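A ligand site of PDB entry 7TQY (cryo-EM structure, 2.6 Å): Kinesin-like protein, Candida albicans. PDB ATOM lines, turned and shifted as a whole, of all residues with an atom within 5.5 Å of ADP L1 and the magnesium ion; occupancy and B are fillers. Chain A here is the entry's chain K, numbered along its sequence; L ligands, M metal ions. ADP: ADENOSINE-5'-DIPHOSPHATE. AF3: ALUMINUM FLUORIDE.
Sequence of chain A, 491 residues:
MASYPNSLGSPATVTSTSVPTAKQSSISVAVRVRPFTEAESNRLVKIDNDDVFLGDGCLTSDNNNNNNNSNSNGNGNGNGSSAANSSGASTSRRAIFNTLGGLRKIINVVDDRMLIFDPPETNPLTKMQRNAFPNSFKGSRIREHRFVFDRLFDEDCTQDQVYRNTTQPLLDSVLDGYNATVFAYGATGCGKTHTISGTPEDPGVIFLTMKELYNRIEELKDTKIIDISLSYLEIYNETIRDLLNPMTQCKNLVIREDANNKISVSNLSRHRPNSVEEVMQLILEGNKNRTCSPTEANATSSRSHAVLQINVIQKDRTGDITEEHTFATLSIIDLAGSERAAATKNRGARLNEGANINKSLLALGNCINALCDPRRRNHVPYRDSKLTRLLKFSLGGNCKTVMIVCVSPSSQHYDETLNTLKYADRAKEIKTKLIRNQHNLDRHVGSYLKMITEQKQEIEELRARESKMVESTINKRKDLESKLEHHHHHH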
ATOM      1  N   ARG A  32     -22.745 -27.919   3.066  1.00  0.00           N
ATOM      2  CA  ARG A  32     -22.886 -28.758   4.248  1.00  0.00           C
ATOM      3  C   ARG A  32     -24.086 -29.681   4.060  1.00  0.00           C
ATOM      4  O   ARG A  32     -25.177 -29.222   3.689  1.00  0.00           O
ATOM      5  CB  ARG A  32     -23.074 -27.902   5.500  1.00  0.00           C
ATOM      6  CG  ARG A  32     -23.034 -28.703   6.793  1.00  0.00           C
ATOM      7  CD  ARG A  32     -23.131 -27.822   8.023  1.00  0.00           C
ATOM      8  NE  ARG A  32     -22.784 -28.551   9.236  1.00  0.00           N
ATOM      9  CZ  ARG A  32     -22.812 -28.047  10.469  1.00  0.00           C
ATOM     10  NH1 ARG A  32     -23.172 -26.791  10.697  1.00  0.00           N
ATOM     11  NH2 ARG A  32     -22.476 -28.818  11.498  1.00  0.00           N
ATOM     12  N   VAL A  33     -23.882 -30.969   4.318  1.00  0.00           N
ATOM     13  CA  VAL A  33     -24.921 -31.987   4.208  1.00  0.00           C
ATOM     14  C   VAL A  33     -25.372 -32.331   5.625  1.00  0.00           C
ATOM     15  O   VAL A  33     -24.560 -32.806   6.432  1.00  0.00           O
ATOM     16  CB  VAL A  33     -24.410 -33.239   3.487  1.00  0.00           C
ATOM     17  CG1 VAL A  33     -25.529 -34.259   3.326  1.00  0.00           C
ATOM     18  CG2 VAL A  33     -23.796 -32.888   2.125  1.00  0.00           C
ATOM     19  N   ARG A  34     -26.661 -32.102   5.931  1.00  0.00           N
ATOM     20  CA  ARG A  34     -27.103 -32.382   7.284  1.00  0.00           C
ATOM     21  C   ARG A  34     -27.314 -33.891   7.482  1.00  0.00           C
ATOM     22  O   ARG A  34     -27.562 -34.608   6.508  1.00  0.00           O
ATOM     23  CB  ARG A  34     -28.383 -31.617   7.614  1.00  0.00           C
ATOM     24  CG  ARG A  34     -29.663 -32.037   6.868  1.00  0.00           C
ATOM     25  CD  ARG A  34     -30.891 -31.713   7.715  1.00  0.00           C
ATOM     26  NE  ARG A  34     -32.142 -31.990   7.009  1.00  0.00           N
ATOM     27  CZ  ARG A  34     -32.714 -33.187   6.910  1.00  0.00           C
ATOM     28  NH1 ARG A  34     -32.173 -34.268   7.428  1.00  0.00           N
ATOM     29  NH2 ARG A  34     -33.871 -33.285   6.258  1.00  0.00           N
ATOM     30  N   PRO A  35     -27.218 -34.391   8.712  1.00  0.00           N
ATOM     31  CA  PRO A  35     -27.488 -35.814   8.942  1.00  0.00           C
ATOM     32  C   PRO A  35     -28.982 -36.107   8.935  1.00  0.00           C
ATOM     33  O   PRO A  35     -29.827 -35.221   9.071  1.00  0.00           O
ATOM     34  CB  PRO A  35     -26.863 -36.078  10.318  1.00  0.00           C
ATOM     35  CG  PRO A  35     -26.997 -34.783  11.010  1.00  0.00           C
ATOM     36  CD  PRO A  35     -26.789 -33.721   9.958  1.00  0.00           C
ATOM     37  N   GLU A 155     -22.144 -35.688   6.605  1.00  0.00           N
ATOM     38  CA  GLU A 155     -23.082 -35.741   7.725  1.00  0.00           C
ATOM     39  C   GLU A 155     -22.353 -35.732   9.064  1.00  0.00           C
ATOM     40  O   GLU A 155     -22.910 -35.239  10.058  1.00  0.00           O
ATOM     41  CB  GLU A 155     -23.976 -36.986   7.641  1.00  0.00           C
ATOM     42  CG  GLU A 155     -24.297 -37.562   6.257  1.00  0.00           C
ATOM     43  CD  GLU A 155     -25.168 -38.800   6.333  1.00  0.00           C
ATOM     44  OE1 GLU A 155     -26.171 -38.787   7.068  1.00  0.00           O
ATOM     45  OE2 GLU A 155     -24.849 -39.797   5.648  1.00  0.00           O
ATOM     46  N   CYS A 157     -19.599 -34.178  10.026  1.00  0.00           N
ATOM     47  CA  CYS A 157     -18.853 -32.991  10.413  1.00  0.00           C
ATOM     48  C   CYS A 157     -19.452 -32.369  11.676  1.00  0.00           C
ATOM     49  O   CYS A 157     -20.640 -32.516  11.968  1.00  0.00           O
ATOM     50  CB  CYS A 157     -18.852 -31.954   9.286  1.00  0.00           C
ATOM     51  SG  CYS A 157     -20.159 -30.720   9.444  1.00  0.00           S
ATOM     52  N   GLN A 159     -19.269 -28.632  14.335  1.00  0.00           N
ATOM     53  CA  GLN A 159     -19.293 -27.187  14.155  1.00  0.00           C
ATOM     54  C   GLN A 159     -17.898 -26.594  13.990  1.00  0.00           C
ATOM     55  O   GLN A 159     -17.718 -25.654  13.218  1.00  0.00           O
ATOM     56  CB  GLN A 159     -19.998 -26.534  15.348  1.00  0.00           C
ATOM     57  CG  GLN A 159     -21.442 -26.986  15.563  1.00  0.00           C
ATOM     58  CD  GLN A 159     -22.386 -26.493  14.486  1.00  0.00           C
ATOM     59  OE1 GLN A 159     -22.301 -26.916  13.332  1.00  0.00           O
ATOM     60  NE2 GLN A 159     -23.307 -25.621  14.860  1.00  0.00           N
ATOM     61  N   ALA A 187     -32.685 -25.028   1.415  1.00  0.00           N
ATOM     62  CA  ALA A 187     -34.093 -25.331   1.616  1.00  0.00           C
ATOM     63  C   ALA A 187     -34.411 -25.422   3.104  1.00  0.00           C
ATOM     64  O   ALA A 187     -33.523 -25.444   3.957  1.00  0.00           O
ATOM     65  CB  ALA A 187     -34.449 -26.647   0.913  1.00  0.00           C
ATOM     66  N   THR A 188     -35.704 -25.448   3.407  1.00  0.00           N
ATOM     67  CA  THR A 188     -36.139 -25.476   4.801  1.00  0.00           C
ATOM     68  C   THR A 188     -35.702 -26.775   5.478  1.00  0.00           C
ATOM     69  O   THR A 188     -35.732 -27.850   4.880  1.00  0.00           O
ATOM     70  CB  THR A 188     -37.660 -25.318   4.895  1.00  0.00           C
ATOM     71  OG1 THR A 188     -38.070 -25.499   6.256  1.00  0.00           O
ATOM     72  CG2 THR A 188     -38.411 -26.336   4.015  1.00  0.00           C
ATOM     73  N   GLY A 189     -35.280 -26.644   6.737  1.00  0.00           N
ATOM     74  CA  GLY A 189     -34.909 -27.806   7.514  1.00  0.00           C
ATOM     75  C   GLY A 189     -33.579 -28.423   7.167  1.00  0.00           C
ATOM     76  O   GLY A 189     -33.371 -29.610   7.439  1.00  0.00           O
ATOM     77  N   CYS A 190     -32.654 -27.651   6.581  1.00  0.00           N
ATOM     78  CA  CYS A 190     -31.368 -28.174   6.133  1.00  0.00           C
ATOM     79  C   CYS A 190     -30.216 -27.867   7.084  1.00  0.00           C
ATOM     80  O   CYS A 190     -29.107 -28.374   6.865  1.00  0.00           O
ATOM     81  CB  CYS A 190     -31.033 -27.616   4.741  1.00  0.00           C
ATOM     82  SG  CYS A 190     -32.140 -28.196   3.441  1.00  0.00           S
ATOM     83  N   GLY A 191     -30.438 -27.047   8.113  1.00  0.00           N
ATOM     84  CA  GLY A 191     -29.439 -26.840   9.150  1.00  0.00           C
ATOM     85  C   GLY A 191     -28.667 -25.531   9.040  1.00  0.00           C
ATOM     86  O   GLY A 191     -27.456 -25.500   9.265  1.00  0.00           O
ATOM     87  N   LYS A 192     -29.368 -24.448   8.688  1.00  0.00           N
ATOM     88  CA  LYS A 192     -28.748 -23.137   8.616  1.00  0.00           C
ATOM     89  C   LYS A 192     -28.654 -22.485   9.984  1.00  0.00           C
ATOM     90  O   LYS A 192     -27.591 -21.982  10.372  1.00  0.00           O
ATOM     91  CB  LYS A 192     -29.524 -22.244   7.665  1.00  0.00           C
ATOM     92  CG  LYS A 192     -29.488 -22.693   6.234  1.00  0.00           C
ATOM     93  CD  LYS A 192     -30.326 -21.790   5.380  1.00  0.00           C
ATOM     94  CE  LYS A 192     -31.747 -22.292   5.321  1.00  0.00           C
ATOM     95  NZ  LYS A 192     -32.656 -21.235   4.832  1.00  0.00           N
ATOM     96  N   THR A 193     -29.765 -22.442  10.718  1.00  0.00           N
ATOM     97  CA  THR A 193     -29.736 -21.902  12.067  1.00  0.00           C
ATOM     98  C   THR A 193     -28.835 -22.724  12.968  1.00  0.00           C
ATOM     99  O   THR A 193     -28.186 -22.189  13.874  1.00  0.00           O
ATOM    100  CB  THR A 193     -31.155 -21.837  12.637  1.00  0.00           C
ATOM    101  OG1 THR A 193     -31.990 -21.075  11.752  1.00  0.00           O
ATOM    102  CG2 THR A 193     -31.166 -21.187  13.999  1.00  0.00           C
ATOM    103  N   HIS A 194     -28.771 -24.031  12.724  1.00  0.00           N
ATOM    104  CA  HIS A 194     -27.831 -24.875  13.451  1.00  0.00           C
ATOM    105  C   HIS A 194     -26.386 -24.489  13.148  1.00  0.00           C
ATOM    106  O   HIS A 194     -25.539 -24.447  14.050  1.00  0.00           O
ATOM    107  CB  HIS A 194     -28.069 -26.348  13.086  1.00  0.00           C
ATOM    108  CG  HIS A 194     -27.225 -27.303  13.872  1.00  0.00           C
ATOM    109  ND1 HIS A 194     -27.538 -27.690  15.161  1.00  0.00           N
ATOM    110  CD2 HIS A 194     -26.090 -27.960  13.550  1.00  0.00           C
ATOM    111  CE1 HIS A 194     -26.629 -28.535  15.592  1.00  0.00           C
ATOM    112  NE2 HIS A 194     -25.736 -28.723  14.639  1.00  0.00           N
ATOM    113  N   THR A 195     -26.088 -24.205  11.886  1.00  0.00           N
ATOM    114  CA  THR A 195     -24.730 -23.835  11.513  1.00  0.00           C
ATOM    115  C   THR A 195     -24.344 -22.483  12.097  1.00  0.00           C
ATOM    116  O   THR A 195     -23.243 -22.316  12.635  1.00  0.00           O
ATOM    117  CB  THR A 195     -24.580 -23.824   9.996  1.00  0.00           C
ATOM    118  OG1 THR A 195     -24.828 -25.133   9.471  1.00  0.00           O
ATOM    119  CG2 THR A 195     -23.181 -23.386   9.593  1.00  0.00           C
ATOM    120  N   ASP A 202     -24.142 -27.161  21.509  1.00  0.00           N
ATOM    121  CA  ASP A 202     -23.360 -27.261  20.291  1.00  0.00           C
ATOM    122  C   ASP A 202     -23.320 -25.893  19.615  1.00  0.00           C
ATOM    123  O   ASP A 202     -24.078 -25.656  18.666  1.00  0.00           O
ATOM    124  CB  ASP A 202     -23.949 -28.324  19.369  1.00  0.00           C
ATOM    125  CG  ASP A 202     -23.009 -28.717  18.241  1.00  0.00           C
ATOM    126  OD1 ASP A 202     -21.824 -28.317  18.272  1.00  0.00           O
ATOM    127  OD2 ASP A 202     -23.457 -29.427  17.311  1.00  0.00           O
ATOM    128  N   ARG A 290     -36.551 -13.294  17.650  1.00  0.00           N
ATOM    129  CA  ARG A 290     -36.798 -13.667  16.263  1.00  0.00           C
ATOM    130  C   ARG A 290     -38.171 -14.322  16.126  1.00  0.00           C
ATOM    131  O   ARG A 290     -38.644 -14.994  17.043  1.00  0.00           O
ATOM    132  CB  ARG A 290     -35.727 -14.640  15.766  1.00  0.00           C
ATOM    133  CG  ARG A 290     -34.380 -14.004  15.497  1.00  0.00           C
ATOM    134  CD  ARG A 290     -33.450 -14.974  14.780  1.00  0.00           C
ATOM    135  NE  ARG A 290     -33.874 -15.240  13.416  1.00  0.00           N
ATOM    136  CZ  ARG A 290     -33.295 -16.107  12.599  1.00  0.00           C
ATOM    137  NH1 ARG A 290     -32.254 -16.836  12.972  1.00  0.00           N
ATOM    138  NH2 ARG A 290     -33.765 -16.246  11.357  1.00  0.00           N
ATOM    139  N   ASN A 298     -39.947 -28.437  10.429  1.00  0.00           N
ATOM    140  CA  ASN A 298     -39.232 -28.550  11.693  1.00  0.00           C
ATOM    141  C   ASN A 298     -39.992 -27.712  12.714  1.00  0.00           C
ATOM    142  O   ASN A 298     -40.556 -26.672  12.389  1.00  0.00           O
ATOM    143  CB  ASN A 298     -37.770 -28.087  11.563  1.00  0.00           C
ATOM    144  CG  ASN A 298     -37.639 -26.742  10.880  1.00  0.00           C
ATOM    145  OD1 ASN A 298     -37.906 -25.702  11.475  1.00  0.00           O
ATOM    146  ND2 ASN A 298     -37.222 -26.757   9.621  1.00  0.00           N
ATOM    147  N   THR A 300     -39.133 -25.778  14.997  1.00  0.00           N
ATOM    148  CA  THR A 300     -38.614 -24.418  15.210  1.00  0.00           C
ATOM    149  C   THR A 300     -38.076 -23.904  13.876  1.00  0.00           C
ATOM    150  O   THR A 300     -36.893 -24.038  13.563  1.00  0.00           O
ATOM    151  CB  THR A 300     -37.532 -24.421  16.286  1.00  0.00           C
ATOM    152  OG1 THR A 300     -36.485 -25.328  15.922  1.00  0.00           O
ATOM    153  CG2 THR A 300     -38.110 -24.827  17.633  1.00  0.00           C
ATOM    154  N   SER A 301     -38.969 -23.293  13.087  1.00  0.00           N
ATOM    155  CA  SER A 301     -38.640 -22.829  11.753  1.00  0.00           C
ATOM    156  C   SER A 301     -38.499 -21.312  11.755  1.00  0.00           C
ATOM    157  O   SER A 301     -39.401 -20.600  12.211  1.00  0.00           O
ATOM    158  CB  SER A 301     -39.719 -23.247  10.749  1.00  0.00           C
ATOM    159  OG  SER A 301     -39.341 -22.883   9.435  1.00  0.00           O
ATOM    160  N   SER A 302     -37.364 -20.820  11.259  1.00  0.00           N
ATOM    161  CA  SER A 302     -37.166 -19.390  11.142  1.00  0.00           C
ATOM    162  C   SER A 302     -38.028 -18.832  10.023  1.00  0.00           C
ATOM    163  O   SER A 302     -38.050 -19.358   8.910  1.00  0.00           O
ATOM    164  CB  SER A 302     -35.692 -19.092  10.861  1.00  0.00           C
ATOM    165  OG  SER A 302     -34.858 -19.717  11.814  1.00  0.00           O
ATOM    166  N   ASP A 334     -28.379 -15.304   8.397  1.00  0.00           N
ATOM    167  CA  ASP A 334     -29.139 -16.549   8.373  1.00  0.00           C
ATOM    168  C   ASP A 334     -30.406 -16.277   7.570  1.00  0.00           C
ATOM    169  O   ASP A 334     -31.230 -15.447   7.959  1.00  0.00           O
ATOM    170  CB  ASP A 334     -29.454 -17.020   9.785  1.00  0.00           C
ATOM    171  CG  ASP A 334     -30.285 -18.297   9.829  1.00  0.00           C
ATOM    172  OD1 ASP A 334     -30.549 -18.896   8.764  1.00  0.00           O
ATOM    173  OD2 ASP A 334     -30.685 -18.695  10.941  1.00  0.00           O
ATOM    174  N   LEU A 335     -30.547 -16.969   6.439  1.00  0.00           N
ATOM    175  CA  LEU A 335     -31.696 -16.810   5.564  1.00  0.00           C
ATOM    176  C   LEU A 335     -32.744 -17.881   5.833  1.00  0.00           C
ATOM    177  O   LEU A 335     -32.413 -19.042   6.092  1.00  0.00           O
ATOM    178  CB  LEU A 335     -31.266 -16.874   4.097  1.00  0.00           C
ATOM    179  CG  LEU A 335     -30.182 -15.902   3.634  1.00  0.00           C
ATOM    180  CD1 LEU A 335     -29.853 -16.143   2.170  1.00  0.00           C
ATOM    181  CD2 LEU A 335     -30.613 -14.459   3.849  1.00  0.00           C
ATOM    182  N   GLY A 337     -35.687 -20.492   4.707  1.00  0.00           N
ATOM    183  CA  GLY A 337     -35.583 -21.493   3.670  1.00  0.00           C
ATOM    184  C   GLY A 337     -36.699 -21.462   2.652  1.00  0.00           C
ATOM    185  O   GLY A 337     -37.825 -21.039   2.937  1.00  0.00           O
HETATM  186  PB  ADP L   1     -33.271 -24.224   9.194  1.00  0.00           P
HETATM  187  O1B ADP L   1     -34.402 -24.248   8.190  1.00  0.00           O
HETATM  188  O2B ADP L   1     -33.393 -23.120  10.221  1.00  0.00           O
HETATM  189  O3B ADP L   1     -31.905 -24.363   8.585  1.00  0.00           O
HETATM  190  PA  ADP L   1     -32.790 -25.748  11.483  1.00  0.00           P
HETATM  191  O1A ADP L   1     -31.351 -25.303  11.383  1.00  0.00           O
HETATM  192  O2A ADP L   1     -33.712 -25.085  12.470  1.00  0.00           O
HETATM  193  O3A ADP L   1     -33.451 -25.579  10.025  1.00  0.00           O
HETATM  194  O5' ADP L   1     -32.807 -27.344  11.685  1.00  0.00           O
HETATM  195  C5' ADP L   1     -33.809 -28.025  12.449  1.00  0.00           C
HETATM  196  C4' ADP L   1     -33.183 -29.225  13.149  1.00  0.00           C
HETATM  197  O4' ADP L   1     -32.208 -29.865  12.321  1.00  0.00           O
HETATM  198  C3' ADP L   1     -32.462 -28.820  14.431  1.00  0.00           C
HETATM  199  O3' ADP L   1     -33.226 -29.212  15.580  1.00  0.00           O
HETATM  200  C2' ADP L   1     -31.127 -29.522  14.392  1.00  0.00           C
HETATM  201  O2' ADP L   1     -30.938 -30.327  15.560  1.00  0.00           O
HETATM  202  C1' ADP L   1     -31.152 -30.375  13.140  1.00  0.00           C
HETATM  203  N9  ADP L   1     -29.837 -30.307  12.452  1.00  0.00           N
HETATM  204  C8  ADP L   1     -29.575 -29.648  11.303  1.00  0.00           C
HETATM  205  N7  ADP L   1     -28.272 -29.810  10.950  1.00  0.00           N
HETATM  206  C5  ADP L   1     -27.682 -30.581  11.885  1.00  0.00           C
HETATM  207  C6  ADP L   1     -26.334 -31.123  12.121  1.00  0.00           C
HETATM  208  N6  ADP L   1     -25.307 -30.876  11.270  1.00  0.00           N
HETATM  209  N1  ADP L   1     -26.145 -31.894  13.225  1.00  0.00           N
HETATM  210  C2  ADP L   1     -27.148 -32.159  14.086  1.00  0.00           C
HETATM  211  N3  ADP L   1     -28.393 -31.682  13.924  1.00  0.00           N
HETATM  212  C4  ADP L   1     -28.724 -30.911  12.863  1.00  0.00           C
HETATM  213 AL   AF3 L   2     -36.275 -22.557   8.041  1.00  0.00          AL
HETATM  214  F1  AF3 L   2     -36.596 -24.165   8.049  1.00  0.00           F
HETATM  215  F2  AF3 L   2     -36.981 -21.587   6.923  1.00  0.00           F
HETATM  216  F3  AF3 L   2     -35.395 -21.895   9.242  1.00  0.00           F
HETATM  217 MG    MG M   1     -34.067 -21.149  10.636  1.00  0.00          MG
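O1A of ADP L1 is in hydrogen-bond range of N of Thr 193, 3.3 Å away. The backbone NH (N) of Lys 192 sits at hydrogen-bond distance from an oxygen (O3B) of ADP L1 (2.5 Å). The backbone NH (N) of Gly 189 lies close to an oxygen (O1B) of ADP L1, 2.9 Å away. An oxygen (O3B) of ADP L1 is in hydrogen-bond range of the backbone NH of Gly 191 (3.1 Å). N of His 194 is in hydrogen-bond range of O1A of ADP L1 (3.2 Å). A ring nitrogen (NE2) of His 194 lies within hydrogen-bond range of a nitrogen (N1) of ADP L1. F3 of AF3 L2 sits close to N of Ser 302 (3.0 Å). N of Gly 189 is in hydrogen-bond range of F1 of AF3 L2 (3.1 Å). The side-chain hydroxyl (OG1) of Thr 188 lies within hydrogen-bond range of a fluorine (F1) of AF3 L2, 2.7 Å away. ND2 of Asn 298 lies within hydrogen-bond range of F1 of AF3 L2, 3.1 Å away. The side-chain hydroxyl of Ser 301 is in hydrogen-bond range of a fluorine (F1) of AF3 L2, at 3.3 Å. A fluorine (F2) of AF3 L2 is in hydrogen-bond range of the backbone NH (N) of Gly 337, at 2.8 Å.
OG of Ser 302 is bound to the magnesium ion (2.0 Å). The magnesium ion is bound by a fluorine (F3) of AF3 L2, at 2.1 Å. An oxygen (O2B) of ADP L1 is bound to the magnesium ion. The side-chain hydroxyl (OG1) of Thr 193 is bound to the magnesium ion, 2.4 Å away. The magnesium ion has four donor atoms within binding distance.
An oxygen (O1B) of ADP L1 binds an aluminium atom (AL) of AF3 L2.
The side-chain hydroxyl (OG1) of Thr 193 lies close to the side-chain carboxylate (OD2) of Asp 334, at 2.8 Å. The side-chain amino group of Lys 192 lies within hydrogen-bond range of the backbone carbonyl oxygen of Leu 335, at 2.5 Å. The backbone carbonyl oxygen (O) of Gly 189 is in hydrogen-bond range of the guanidinium group (NE) of Arg 34 (2.7 Å). SG of Cys 157 sits at hydrogen-bond distance from NE of Arg 32, 3.4 Å away. The side-chain amide oxygen of Gln 159 is in hydrogen-bond range of the guanidinium group of Arg 32, 2.6 Å away. NH1 of Arg 32 sits at hydrogen-bond distance from OG1 of Thr 195, at 2.6 Å. The backbone carbonyl oxygen (O) of Ala 187 lies within hydrogen-bond range of the side-chain sulfur (SG) of Cys 190 (3.1 Å). The side-chain amide oxygen (OD1) of Asn 298 lies close to the backbone NH (N) of Ser 301 (3.1 Å).
Residues that only touch ADP L1: Arg 32 (3.5 Å), Arg 34 (3.8 Å), Pro 35 (3.4 Å), Thr 188 (3.9 Å), Cys 190 (3.9 Å), Asn 298 (3.97 Å) and Thr 300 (3.5 Å). Hydrophobic or aromatic side chains within 4 Å of ADP L1: Pro 35 and His 194. Within 4 Å of ADP L1: Arg 32, Arg 34, Pro 35, Thr 188, Gly 189, Cys 190, Gly 191, Lys 192, Thr 193, His 194, Asn 298 and Thr 300. The nearest printed residue that does not touch ADP L1 is Ser 302 (4.03 Å).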
